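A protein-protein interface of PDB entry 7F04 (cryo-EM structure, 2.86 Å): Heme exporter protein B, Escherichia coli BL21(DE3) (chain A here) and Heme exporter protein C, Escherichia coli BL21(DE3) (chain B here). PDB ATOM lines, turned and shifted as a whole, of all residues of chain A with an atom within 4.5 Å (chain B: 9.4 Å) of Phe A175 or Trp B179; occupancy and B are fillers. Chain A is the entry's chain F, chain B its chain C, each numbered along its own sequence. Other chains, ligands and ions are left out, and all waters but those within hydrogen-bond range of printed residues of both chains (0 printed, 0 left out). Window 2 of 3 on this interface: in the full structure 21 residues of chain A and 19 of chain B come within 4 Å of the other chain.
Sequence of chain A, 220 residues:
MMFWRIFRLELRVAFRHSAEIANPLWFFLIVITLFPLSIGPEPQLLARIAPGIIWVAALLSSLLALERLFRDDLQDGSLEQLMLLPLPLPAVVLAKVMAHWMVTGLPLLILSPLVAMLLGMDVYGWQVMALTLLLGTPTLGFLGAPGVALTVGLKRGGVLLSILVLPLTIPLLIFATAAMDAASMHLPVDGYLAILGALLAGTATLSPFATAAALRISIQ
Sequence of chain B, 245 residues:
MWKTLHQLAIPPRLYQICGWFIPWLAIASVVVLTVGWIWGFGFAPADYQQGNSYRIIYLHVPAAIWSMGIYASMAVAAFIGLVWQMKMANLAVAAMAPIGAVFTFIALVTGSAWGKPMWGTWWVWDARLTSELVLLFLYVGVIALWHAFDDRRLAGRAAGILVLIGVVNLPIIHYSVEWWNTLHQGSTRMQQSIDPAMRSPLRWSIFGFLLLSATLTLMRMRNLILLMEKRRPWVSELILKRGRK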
ATOM      1  N   PRO A 171       7.627  27.197 -20.758  1.00  0.00           N
ATOM      2  CA  PRO A 171       7.916  26.504 -22.027  1.00  0.00           C
ATOM      3  C   PRO A 171       7.145  27.061 -23.211  1.00  0.00           C
ATOM      4  O   PRO A 171       7.696  27.171 -24.315  1.00  0.00           O
ATOM      5  CB  PRO A 171       7.528  25.049 -21.727  1.00  0.00           C
ATOM      6  CG  PRO A 171       6.649  25.113 -20.541  1.00  0.00           C
ATOM      7  CD  PRO A 171       7.160  26.250 -19.731  1.00  0.00           C
ATOM      8  N   LEU A 172       5.879  27.426 -23.005  1.00  0.00           N
ATOM      9  CA  LEU A 172       5.093  28.014 -24.083  1.00  0.00           C
ATOM     10  C   LEU A 172       5.690  29.341 -24.525  1.00  0.00           C
ATOM     11  O   LEU A 172       5.827  29.602 -25.723  1.00  0.00           O
ATOM     12  CB  LEU A 172       3.644  28.196 -23.635  1.00  0.00           C
ATOM     13  CG  LEU A 172       2.809  29.181 -24.452  1.00  0.00           C
ATOM     14  CD1 LEU A 172       2.542  28.628 -25.838  1.00  0.00           C
ATOM     15  CD2 LEU A 172       1.510  29.485 -23.737  1.00  0.00           C
ATOM     16  N   LEU A 173       6.066  30.186 -23.563  1.00  0.00           N
ATOM     17  CA  LEU A 173       6.719  31.450 -23.889  1.00  0.00           C
ATOM     18  C   LEU A 173       8.005  31.220 -24.665  1.00  0.00           C
ATOM     19  O   LEU A 173       8.252  31.876 -25.682  1.00  0.00           O
ATOM     20  CB  LEU A 173       7.011  32.226 -22.605  1.00  0.00           C
ATOM     21  CG  LEU A 173       7.658  33.606 -22.721  1.00  0.00           C
ATOM     22  CD1 LEU A 173       6.760  34.576 -23.459  1.00  0.00           C
ATOM     23  CD2 LEU A 173       8.014  34.139 -21.347  1.00  0.00           C
ATOM     24  N   ILE A 174       8.825  30.274 -24.208  1.00  0.00           N
ATOM     25  CA  ILE A 174      10.124  30.037 -24.827  1.00  0.00           C
ATOM     26  C   ILE A 174       9.948  29.595 -26.272  1.00  0.00           C
ATOM     27  O   ILE A 174      10.563  30.150 -27.188  1.00  0.00           O
ATOM     28  CB  ILE A 174      10.919  29.001 -24.013  1.00  0.00           C
ATOM     29  CG1 ILE A 174      11.531  29.658 -22.776  1.00  0.00           C
ATOM     30  CG2 ILE A 174      11.996  28.357 -24.866  1.00  0.00           C
ATOM     31  CD1 ILE A 174      12.347  28.720 -21.931  1.00  0.00           C
ATOM     32  N   PHE A 175       9.081  28.609 -26.501  1.00  0.00           N
ATOM     33  CA  PHE A 175       8.955  28.068 -27.848  1.00  0.00           C
ATOM     34  C   PHE A 175       8.189  29.007 -28.769  1.00  0.00           C
ATOM     35  O   PHE A 175       8.488  29.072 -29.966  1.00  0.00           O
ATOM     36  CB  PHE A 175       8.308  26.690 -27.791  1.00  0.00           C
ATOM     37  CG  PHE A 175       9.264  25.613 -27.388  1.00  0.00           C
ATOM     38  CD1 PHE A 175      10.280  25.223 -28.239  1.00  0.00           C
ATOM     39  CD2 PHE A 175       9.172  25.017 -26.147  1.00  0.00           C
ATOM     40  CE1 PHE A 175      11.169  24.243 -27.868  1.00  0.00           C
ATOM     41  CE2 PHE A 175      10.059  24.038 -25.771  1.00  0.00           C
ATOM     42  CZ  PHE A 175      11.060  23.652 -26.633  1.00  0.00           C
ATOM     43  N   ALA A 176       7.231  29.767 -28.236  1.00  0.00           N
ATOM     44  CA  ALA A 176       6.534  30.764 -29.035  1.00  0.00           C
ATOM     45  C   ALA A 176       7.482  31.866 -29.489  1.00  0.00           C
ATOM     46  O   ALA A 176       7.497  32.247 -30.668  1.00  0.00           O
ATOM     47  CB  ALA A 176       5.380  31.343 -28.223  1.00  0.00           C
ATOM     48  N   THR A 177       8.286  32.391 -28.561  1.00  0.00           N
ATOM     49  CA  THR A 177       9.248  33.425 -28.918  1.00  0.00           C
ATOM     50  C   THR A 177      10.305  32.885 -29.867  1.00  0.00           C
ATOM     51  O   THR A 177      10.765  33.601 -30.759  1.00  0.00           O
ATOM     52  CB  THR A 177       9.897  33.999 -27.661  1.00  0.00           C
ATOM     53  OG1 THR A 177      10.334  32.928 -26.817  1.00  0.00           O
ATOM     54  CG2 THR A 177       8.907  34.861 -26.902  1.00  0.00           C
ATOM     55  N   ALA A 178      10.712  31.626 -29.688  1.00  0.00           N
ATOM     56  CA  ALA A 178      11.668  31.022 -30.610  1.00  0.00           C
ATOM     57  C   ALA A 178      11.091  30.909 -32.012  1.00  0.00           C
ATOM     58  O   ALA A 178      11.780  31.190 -32.999  1.00  0.00           O
ATOM     59  CB  ALA A 178      12.094  29.652 -30.095  1.00  0.00           C
ATOM     60  N   ALA A 179       9.828  30.492 -32.122  1.00  0.00           N
ATOM     61  CA  ALA A 179       9.179  30.412 -33.426  1.00  0.00           C
ATOM     62  C   ALA A 179       9.115  31.779 -34.087  1.00  0.00           C
ATOM     63  O   ALA A 179       9.452  31.934 -35.268  1.00  0.00           O
ATOM     64  CB  ALA A 179       7.776  29.831 -33.272  1.00  0.00           C
ATOM     65  N   TYR A 192       8.798  24.253 -34.647  1.00  0.00           N
ATOM     66  CA  TYR A 192       8.327  25.045 -33.517  1.00  0.00           C
ATOM     67  C   TYR A 192       6.813  24.978 -33.397  1.00  0.00           C
ATOM     68  O   TYR A 192       6.271  24.837 -32.295  1.00  0.00           O
ATOM     69  CB  TYR A 192       8.786  26.488 -33.688  1.00  0.00           C
ATOM     70  CG  TYR A 192      10.263  26.669 -33.475  1.00  0.00           C
ATOM     71  CD1 TYR A 192      10.871  26.232 -32.314  1.00  0.00           C
ATOM     72  CD2 TYR A 192      11.055  27.249 -34.452  1.00  0.00           C
ATOM     73  CE1 TYR A 192      12.217  26.385 -32.124  1.00  0.00           C
ATOM     74  CE2 TYR A 192      12.406  27.407 -34.269  1.00  0.00           C
ATOM     75  CZ  TYR A 192      12.983  26.974 -33.102  1.00  0.00           C
ATOM     76  OH  TYR A 192      14.336  27.129 -32.912  1.00  0.00           O
ATOM     77  N   ILE A 195       5.872  21.630 -31.980  1.00  0.00           N
ATOM     78  CA  ILE A 195       6.034  21.583 -30.527  1.00  0.00           C
ATOM     79  C   ILE A 195       4.902  22.337 -29.837  1.00  0.00           C
ATOM     80  O   ILE A 195       4.391  21.905 -28.797  1.00  0.00           O
ATOM     81  CB  ILE A 195       7.412  22.136 -30.121  1.00  0.00           C
ATOM     82  CG1 ILE A 195       8.522  21.181 -30.556  1.00  0.00           C
ATOM     83  CG2 ILE A 195       7.479  22.362 -28.623  1.00  0.00           C
ATOM     84  CD1 ILE A 195       9.903  21.771 -30.436  1.00  0.00           C
ATOM     85  N   LEU A 196       4.506  23.484 -30.391  1.00  0.00           N
ATOM     86  CA  LEU A 196       3.406  24.244 -29.806  1.00  0.00           C
ATOM     87  C   LEU A 196       2.098  23.467 -29.875  1.00  0.00           C
ATOM     88  O   LEU A 196       1.304  23.484 -28.926  1.00  0.00           O
ATOM     89  CB  LEU A 196       3.267  25.593 -30.508  1.00  0.00           C
ATOM     90  CG  LEU A 196       4.261  26.671 -30.082  1.00  0.00           C
ATOM     91  CD1 LEU A 196       3.901  27.984 -30.733  1.00  0.00           C
ATOM     92  CD2 LEU A 196       4.282  26.809 -28.573  1.00  0.00           C
ATOM     93  N   ASP B 126      21.706  31.638 -17.257  1.00  0.00           N
ATOM     94  CA  ASP B 126      22.047  30.384 -17.905  1.00  0.00           C
ATOM     95  C   ASP B 126      20.952  29.356 -17.639  1.00  0.00           C
ATOM     96  O   ASP B 126      19.926  29.646 -17.021  1.00  0.00           O
ATOM     97  CB  ASP B 126      23.410  29.879 -17.427  1.00  0.00           C
ATOM     98  CG  ASP B 126      23.561  29.941 -15.923  1.00  0.00           C
ATOM     99  OD1 ASP B 126      22.649  30.468 -15.262  1.00  0.00           O
ATOM    100  OD2 ASP B 126      24.590  29.467 -15.400  1.00  0.00           O
ATOM    101  N   ALA B 127      21.173  28.133 -18.125  1.00  0.00           N
ATOM    102  CA  ALA B 127      20.181  27.079 -17.946  1.00  0.00           C
ATOM    103  C   ALA B 127      20.104  26.628 -16.495  1.00  0.00           C
ATOM    104  O   ALA B 127      19.019  26.313 -15.994  1.00  0.00           O
ATOM    105  CB  ALA B 127      20.499  25.895 -18.856  1.00  0.00           C
ATOM    106  N   SER B 131      16.602  27.149 -14.314  1.00  0.00           N
ATOM    107  CA  SER B 131      15.854  25.965 -13.902  1.00  0.00           C
ATOM    108  C   SER B 131      15.616  25.955 -12.397  1.00  0.00           C
ATOM    109  O   SER B 131      14.506  25.661 -11.935  1.00  0.00           O
ATOM    110  CB  SER B 131      16.594  24.702 -14.337  1.00  0.00           C
ATOM    111  OG  SER B 131      16.660  24.611 -15.749  1.00  0.00           O
ATOM    112  N   PRO B 171       9.432  18.506 -16.004  1.00  0.00           N
ATOM    113  CA  PRO B 171      10.339  18.101 -17.091  1.00  0.00           C
ATOM    114  C   PRO B 171      10.183  18.935 -18.346  1.00  0.00           C
ATOM    115  O   PRO B 171      11.177  19.185 -19.041  1.00  0.00           O
ATOM    116  CB  PRO B 171       9.964  16.633 -17.336  1.00  0.00           C
ATOM    117  CG  PRO B 171       8.614  16.475 -16.760  1.00  0.00           C
ATOM    118  CD  PRO B 171       8.574  17.386 -15.583  1.00  0.00           C
ATOM    119  N   ILE B 172       8.964  19.380 -18.658  1.00  0.00           N
ATOM    120  CA  ILE B 172       8.756  20.239 -19.819  1.00  0.00           C
ATOM    121  C   ILE B 172       9.504  21.553 -19.643  1.00  0.00           C
ATOM    122  O   ILE B 172      10.217  22.009 -20.543  1.00  0.00           O
ATOM    123  CB  ILE B 172       7.252  20.476 -20.047  1.00  0.00           C
ATOM    124  CG1 ILE B 172       6.519  19.147 -20.206  1.00  0.00           C
ATOM    125  CG2 ILE B 172       7.027  21.350 -21.264  1.00  0.00           C
ATOM    126  CD1 ILE B 172       5.028  19.258 -20.020  1.00  0.00           C
ATOM    127  N   ILE B 173       9.363  22.171 -18.468  1.00  0.00           N
ATOM    128  CA  ILE B 173      10.041  23.436 -18.202  1.00  0.00           C
ATOM    129  C   ILE B 173      11.550  23.248 -18.232  1.00  0.00           C
ATOM    130  O   ILE B 173      12.280  24.071 -18.795  1.00  0.00           O
ATOM    131  CB  ILE B 173       9.577  24.026 -16.858  1.00  0.00           C
ATOM    132  CG1 ILE B 173       8.072  24.290 -16.874  1.00  0.00           C
ATOM    133  CG2 ILE B 173      10.320  25.309 -16.561  1.00  0.00           C
ATOM    134  CD1 ILE B 173       7.509  24.674 -15.530  1.00  0.00           C
ATOM    135  N   HIS B 174      12.042  22.169 -17.623  1.00  0.00           N
ATOM    136  CA  HIS B 174      13.483  21.940 -17.585  1.00  0.00           C
ATOM    137  C   HIS B 174      14.047  21.757 -18.986  1.00  0.00           C
ATOM    138  O   HIS B 174      15.076  22.345 -19.334  1.00  0.00           O
ATOM    139  CB  HIS B 174      13.804  20.725 -16.717  1.00  0.00           C
ATOM    140  CG  HIS B 174      15.249  20.335 -16.743  1.00  0.00           C
ATOM    141  ND1 HIS B 174      15.743  19.363 -17.584  1.00  0.00           N
ATOM    142  CD2 HIS B 174      16.306  20.790 -16.031  1.00  0.00           C
ATOM    143  CE1 HIS B 174      17.043  19.236 -17.391  1.00  0.00           C
ATOM    144  NE2 HIS B 174      17.410  20.089 -16.453  1.00  0.00           N
ATOM    145  N   TYR B 175      13.381  20.947 -19.810  1.00  0.00           N
ATOM    146  CA  TYR B 175      13.888  20.703 -21.156  1.00  0.00           C
ATOM    147  C   TYR B 175      13.786  21.954 -22.018  1.00  0.00           C
ATOM    148  O   TYR B 175      14.658  22.206 -22.858  1.00  0.00           O
ATOM    149  CB  TYR B 175      13.135  19.540 -21.798  1.00  0.00           C
ATOM    150  CG  TYR B 175      13.799  18.198 -21.591  1.00  0.00           C
ATOM    151  CD1 TYR B 175      14.083  17.734 -20.314  1.00  0.00           C
ATOM    152  CD2 TYR B 175      14.139  17.396 -22.670  1.00  0.00           C
ATOM    153  CE1 TYR B 175      14.687  16.510 -20.117  1.00  0.00           C
ATOM    154  CE2 TYR B 175      14.743  16.170 -22.485  1.00  0.00           C
ATOM    155  CZ  TYR B 175      15.015  15.731 -21.206  1.00  0.00           C
ATOM    156  OH  TYR B 175      15.619  14.508 -21.018  1.00  0.00           O
ATOM    157  N   SER B 176      12.733  22.752 -21.827  1.00  0.00           N
ATOM    158  CA  SER B 176      12.612  24.003 -22.565  1.00  0.00           C
ATOM    159  C   SER B 176      13.715  24.980 -22.183  1.00  0.00           C
ATOM    160  O   SER B 176      14.279  25.655 -23.050  1.00  0.00           O
ATOM    161  CB  SER B 176      11.240  24.621 -22.318  1.00  0.00           C
ATOM    162  OG  SER B 176      10.216  23.699 -22.639  1.00  0.00           O
ATOM    163  N   VAL B 177      14.034  25.073 -20.892  1.00  0.00           N
ATOM    164  CA  VAL B 177      15.103  25.966 -20.459  1.00  0.00           C
ATOM    165  C   VAL B 177      16.450  25.474 -20.970  1.00  0.00           C
ATOM    166  O   VAL B 177      17.300  26.272 -21.382  1.00  0.00           O
ATOM    167  CB  VAL B 177      15.094  26.114 -18.926  1.00  0.00           C
ATOM    168  CG1 VAL B 177      16.314  26.882 -18.462  1.00  0.00           C
ATOM    169  CG2 VAL B 177      13.833  26.820 -18.473  1.00  0.00           C
ATOM    170  N   GLU B 178      16.672  24.158 -20.953  1.00  0.00           N
ATOM    171  CA  GLU B 178      17.924  23.619 -21.478  1.00  0.00           C
ATOM    172  C   GLU B 178      18.063  23.898 -22.966  1.00  0.00           C
ATOM    173  O   GLU B 178      19.155  24.225 -23.442  1.00  0.00           O
ATOM    174  CB  GLU B 178      18.020  22.120 -21.203  1.00  0.00           C
ATOM    175  CG  GLU B 178      18.129  21.773 -19.735  1.00  0.00           C
ATOM    176  CD  GLU B 178      19.431  22.252 -19.126  1.00  0.00           C
ATOM    177  OE1 GLU B 178      20.447  22.290 -19.852  1.00  0.00           O
ATOM    178  OE2 GLU B 178      19.442  22.594 -17.925  1.00  0.00           O
ATOM    179  N   TRP B 179      16.973  23.766 -23.720  1.00  0.00           N
ATOM    180  CA  TRP B 179      17.040  24.072 -25.142  1.00  0.00           C
ATOM    181  C   TRP B 179      17.089  25.573 -25.395  1.00  0.00           C
ATOM    182  O   TRP B 179      17.696  26.011 -26.378  1.00  0.00           O
ATOM    183  CB  TRP B 179      15.852  23.448 -25.870  1.00  0.00           C
ATOM    184  CG  TRP B 179      15.783  23.831 -27.304  1.00  0.00           C
ATOM    185  CD1 TRP B 179      16.353  23.180 -28.356  1.00  0.00           C
ATOM    186  CD2 TRP B 179      15.114  24.967 -27.849  1.00  0.00           C
ATOM    187  NE1 TRP B 179      16.077  23.840 -29.524  1.00  0.00           N
ATOM    188  CE2 TRP B 179      15.318  24.942 -29.238  1.00  0.00           C
ATOM    189  CE3 TRP B 179      14.362  26.006 -27.294  1.00  0.00           C
ATOM    190  CZ2 TRP B 179      14.798  25.911 -30.080  1.00  0.00           C
ATOM    191  CZ3 TRP B 179      13.848  26.966 -28.130  1.00  0.00           C
ATOM    192  CH2 TRP B 179      14.067  26.913 -29.507  1.00  0.00           C
ATOM    193  N   TRP B 180      16.462  26.371 -24.527  1.00  0.00           N
ATOM    194  CA  TRP B 180      16.536  27.824 -24.655  1.00  0.00           C
ATOM    195  C   TRP B 180      17.961  28.323 -24.486  1.00  0.00           C
ATOM    196  O   TRP B 180      18.355  29.305 -25.124  1.00  0.00           O
ATOM    197  CB  TRP B 180      15.608  28.477 -23.629  1.00  0.00           C
ATOM    198  CG  TRP B 180      15.853  29.932 -23.372  1.00  0.00           C
ATOM    199  CD1 TRP B 180      15.392  30.981 -24.109  1.00  0.00           C
ATOM    200  CD2 TRP B 180      16.586  30.502 -22.280  1.00  0.00           C
ATOM    201  NE1 TRP B 180      15.806  32.168 -23.556  1.00  0.00           N
ATOM    202  CE2 TRP B 180      16.541  31.900 -22.433  1.00  0.00           C
ATOM    203  CE3 TRP B 180      17.285  29.964 -21.197  1.00  0.00           C
ATOM    204  CZ2 TRP B 180      17.167  32.766 -21.543  1.00  0.00           C
ATOM    205  CZ3 TRP B 180      17.905  30.827 -20.315  1.00  0.00           C
ATOM    206  CH2 TRP B 180      17.841  32.212 -20.493  1.00  0.00           C
ATOM    207  N   ASN B 181      18.747  27.667 -23.630  1.00  0.00           N
ATOM    208  CA  ASN B 181      20.140  28.058 -23.446  1.00  0.00           C
ATOM    209  C   ASN B 181      20.976  27.745 -24.679  1.00  0.00           C
ATOM    210  O   ASN B 181      21.791  28.570 -25.105  1.00  0.00           O
ATOM    211  CB  ASN B 181      20.719  27.357 -22.219  1.00  0.00           C
ATOM    212  CG  ASN B 181      21.832  28.146 -21.572  1.00  0.00           C
ATOM    213  OD1 ASN B 181      21.912  29.364 -21.721  1.00  0.00           O
ATOM    214  ND2 ASN B 181      22.700  27.456 -20.846  1.00  0.00           N
ATOM    215  N   THR B 182      20.800  26.557 -25.261  1.00  0.00           N
ATOM    216  CA  THR B 182      21.570  26.199 -26.447  1.00  0.00           C
ATOM    217  C   THR B 182      21.198  27.067 -27.636  1.00  0.00           C
ATOM    218  O   THR B 182      22.024  27.283 -28.530  1.00  0.00           O
ATOM    219  CB  THR B 182      21.362  24.728 -26.795  1.00  0.00           C
ATOM    220  OG1 THR B 182      20.028  24.537 -27.279  1.00  0.00           O
ATOM    221  CG2 THR B 182      21.588  23.850 -25.574  1.00  0.00           C
ATOM    222  N   LEU B 183      19.962  27.564 -27.670  1.00  0.00           N
ATOM    223  CA  LEU B 183      19.544  28.447 -28.750  1.00  0.00           C
ATOM    224  C   LEU B 183      20.307  29.764 -28.724  1.00  0.00           C
ATOM    225  O   LEU B 183      20.434  30.426 -29.758  1.00  0.00           O
ATOM    226  CB  LEU B 183      18.041  28.703 -28.655  1.00  0.00           C
ATOM    227  CG  LEU B 183      17.370  29.388 -29.840  1.00  0.00           C
ATOM    228  CD1 LEU B 183      17.352  28.463 -31.042  1.00  0.00           C
ATOM    229  CD2 LEU B 183      15.968  29.827 -29.470  1.00  0.00           C
ATOM    230  N   HIS B 184      20.822  30.155 -27.560  1.00  0.00           N
ATOM    231  CA  HIS B 184      21.505  31.431 -27.395  1.00  0.00           C
ATOM    232  C   HIS B 184      23.018  31.286 -27.275  1.00  0.00           C
ATOM    233  O   HIS B 184      23.758  31.937 -28.017  1.00  0.00           O
ATOM    234  CB  HIS B 184      20.943  32.164 -26.172  1.00  0.00           C
ATOM    235  CG  HIS B 184      19.597  32.775 -26.404  1.00  0.00           C
ATOM    236  ND1 HIS B 184      18.460  32.340 -25.761  1.00  0.00           N
ATOM    237  CD2 HIS B 184      19.206  33.787 -27.215  1.00  0.00           C
ATOM    238  CE1 HIS B 184      17.426  33.055 -26.164  1.00  0.00           C
ATOM    239  NE2 HIS B 184      17.852  33.941 -27.047  1.00  0.00           N
ATOM    240  N   GLN B 185      23.503  30.443 -26.365  1.00  0.00           N
ATOM    241  CA  GLN B 185      24.939  30.303 -26.155  1.00  0.00           C
ATOM    242  C   GLN B 185      25.496  28.947 -26.564  1.00  0.00           C
ATOM    243  O   GLN B 185      26.535  28.897 -27.226  1.00  0.00           O
ATOM    244  CB  GLN B 185      25.290  30.599 -24.691  1.00  0.00           C
ATOM    245  CG  GLN B 185      24.596  29.733 -23.664  1.00  0.00           C
ATOM    246  CD  GLN B 185      25.455  28.571 -23.230  1.00  0.00           C
ATOM    247  OE1 GLN B 185      26.682  28.662 -23.221  1.00  0.00           O
ATOM    248  NE2 GLN B 185      24.816  27.468 -22.865  1.00  0.00           N
ATOM    249  N   GLY B 186      24.848  27.840 -26.203  1.00  0.00           N
ATOM    250  CA  GLY B 186      25.223  26.559 -26.775  1.00  0.00           C
ATOM    251  C   GLY B 186      25.392  25.357 -25.863  1.00  0.00           C
ATOM    252  O   GLY B 186      24.939  24.266 -26.222  1.00  0.00           O
ATOM    253  N   SER B 187      26.018  25.511 -24.701  1.00  0.00           N
ATOM    254  CA  SER B 187      26.314  24.361 -23.843  1.00  0.00           C
ATOM    255  C   SER B 187      26.703  24.865 -22.455  1.00  0.00           C
ATOM    256  O   SER B 187      26.583  26.057 -22.151  1.00  0.00           O
ATOM    257  CB  SER B 187      27.414  23.486 -24.452  1.00  0.00           C
ATOM    258  OG  SER B 187      28.535  24.265 -24.831  1.00  0.00           O
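Printed residues of chain B within 4 Å of Pro A171: Ile B172, Ile B173 and Ser B176.
Phe A175 touches just these residues of chain B: Ser B176 (3.2 Å) and Trp B179 (3.7 Å).
No residue of chain B comes within 4 Å of Ala A176.
Of the printed residues of chain B, Ala A178 touches Trp B179 and Leu B183.
Printed residues of chain A within 4 Å of Leu B183: Ala A178 and Tyr A192.
The nearest residue of chain B that does not touch Phe A175 is Tyr B175 (5.4 Å).
The nearest printed residue of chain A that does not touch Trp B179 is Ile A174 (4.002 Å).
The nearest printed residue of chain B that does not touch Ile A174 is Trp B179 (4.002 Å).
The backbone carbonyl oxygen (O) of Ile A174 is in hydrogen-bond range of the side-chain hydroxyl (OG1) of Thr A177, 2.8 Å away.
The side-chain hydroxyl (OG1) of Thr B182 is in hydrogen-bond range of the backbone carbonyl oxygen (O) of Trp B179 (2.9 Å).
The backbone carbonyl oxygen of Trp B180 is in hydrogen-bond range of a ring nitrogen (ND1) of His B184 (3.1 Å).
The backbone carbonyl oxygen of Ile B172 sits at hydrogen-bond distance from the side-chain hydroxyl of Ser B176.
Hydrophobic or aromatic side chains of chain A within 4 Å of the printed part of chain B: Pro A171, Ile A174, Phe A175, Ala A178 and Tyr A192.
Printed residues of chain B that touch a printed residue of chain A: Ile B172, Ile B173, Ser B176, Trp B179, Trp B180 and Leu B183.
Hydrophobic or aromatic side chains of chain B that line the printed part of chain A: Ile B172, Ile B173, Trp B179, Trp B180 and Leu B183.
Along chain B the printed residues that touch a printed residue of chain A span positions 172 to 183.
Among the printed residues, 11 pairs touch across the chains.
Among the printed residues, no Asp or Glu carboxylate lies within 4 Å of a Lys or Arg side-chain nitrogen of the other chain.
Among the printed residues, merely in contact across the chains: Pro A171 with Ile B172 (3.8 Å), Pro A171 with Ile B173 (3.6 Å), Pro A171 with Ser B176 (3.1 Å), Ile A174 with Ser B176 (3.8 Å), Ile A174 with Trp B180 (3.7 Å), Phe A175 with Ser B176 (3.2 Å), Phe A175 with Trp B179 (3.7 Å), Ala A178 with Trp B179 (3.4 Å), Ala A178 with Leu B183 (3.9 Å), Tyr A192 with Trp B179 (3.1 Å) and Tyr A192 with Leu B183 (3.8 Å).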
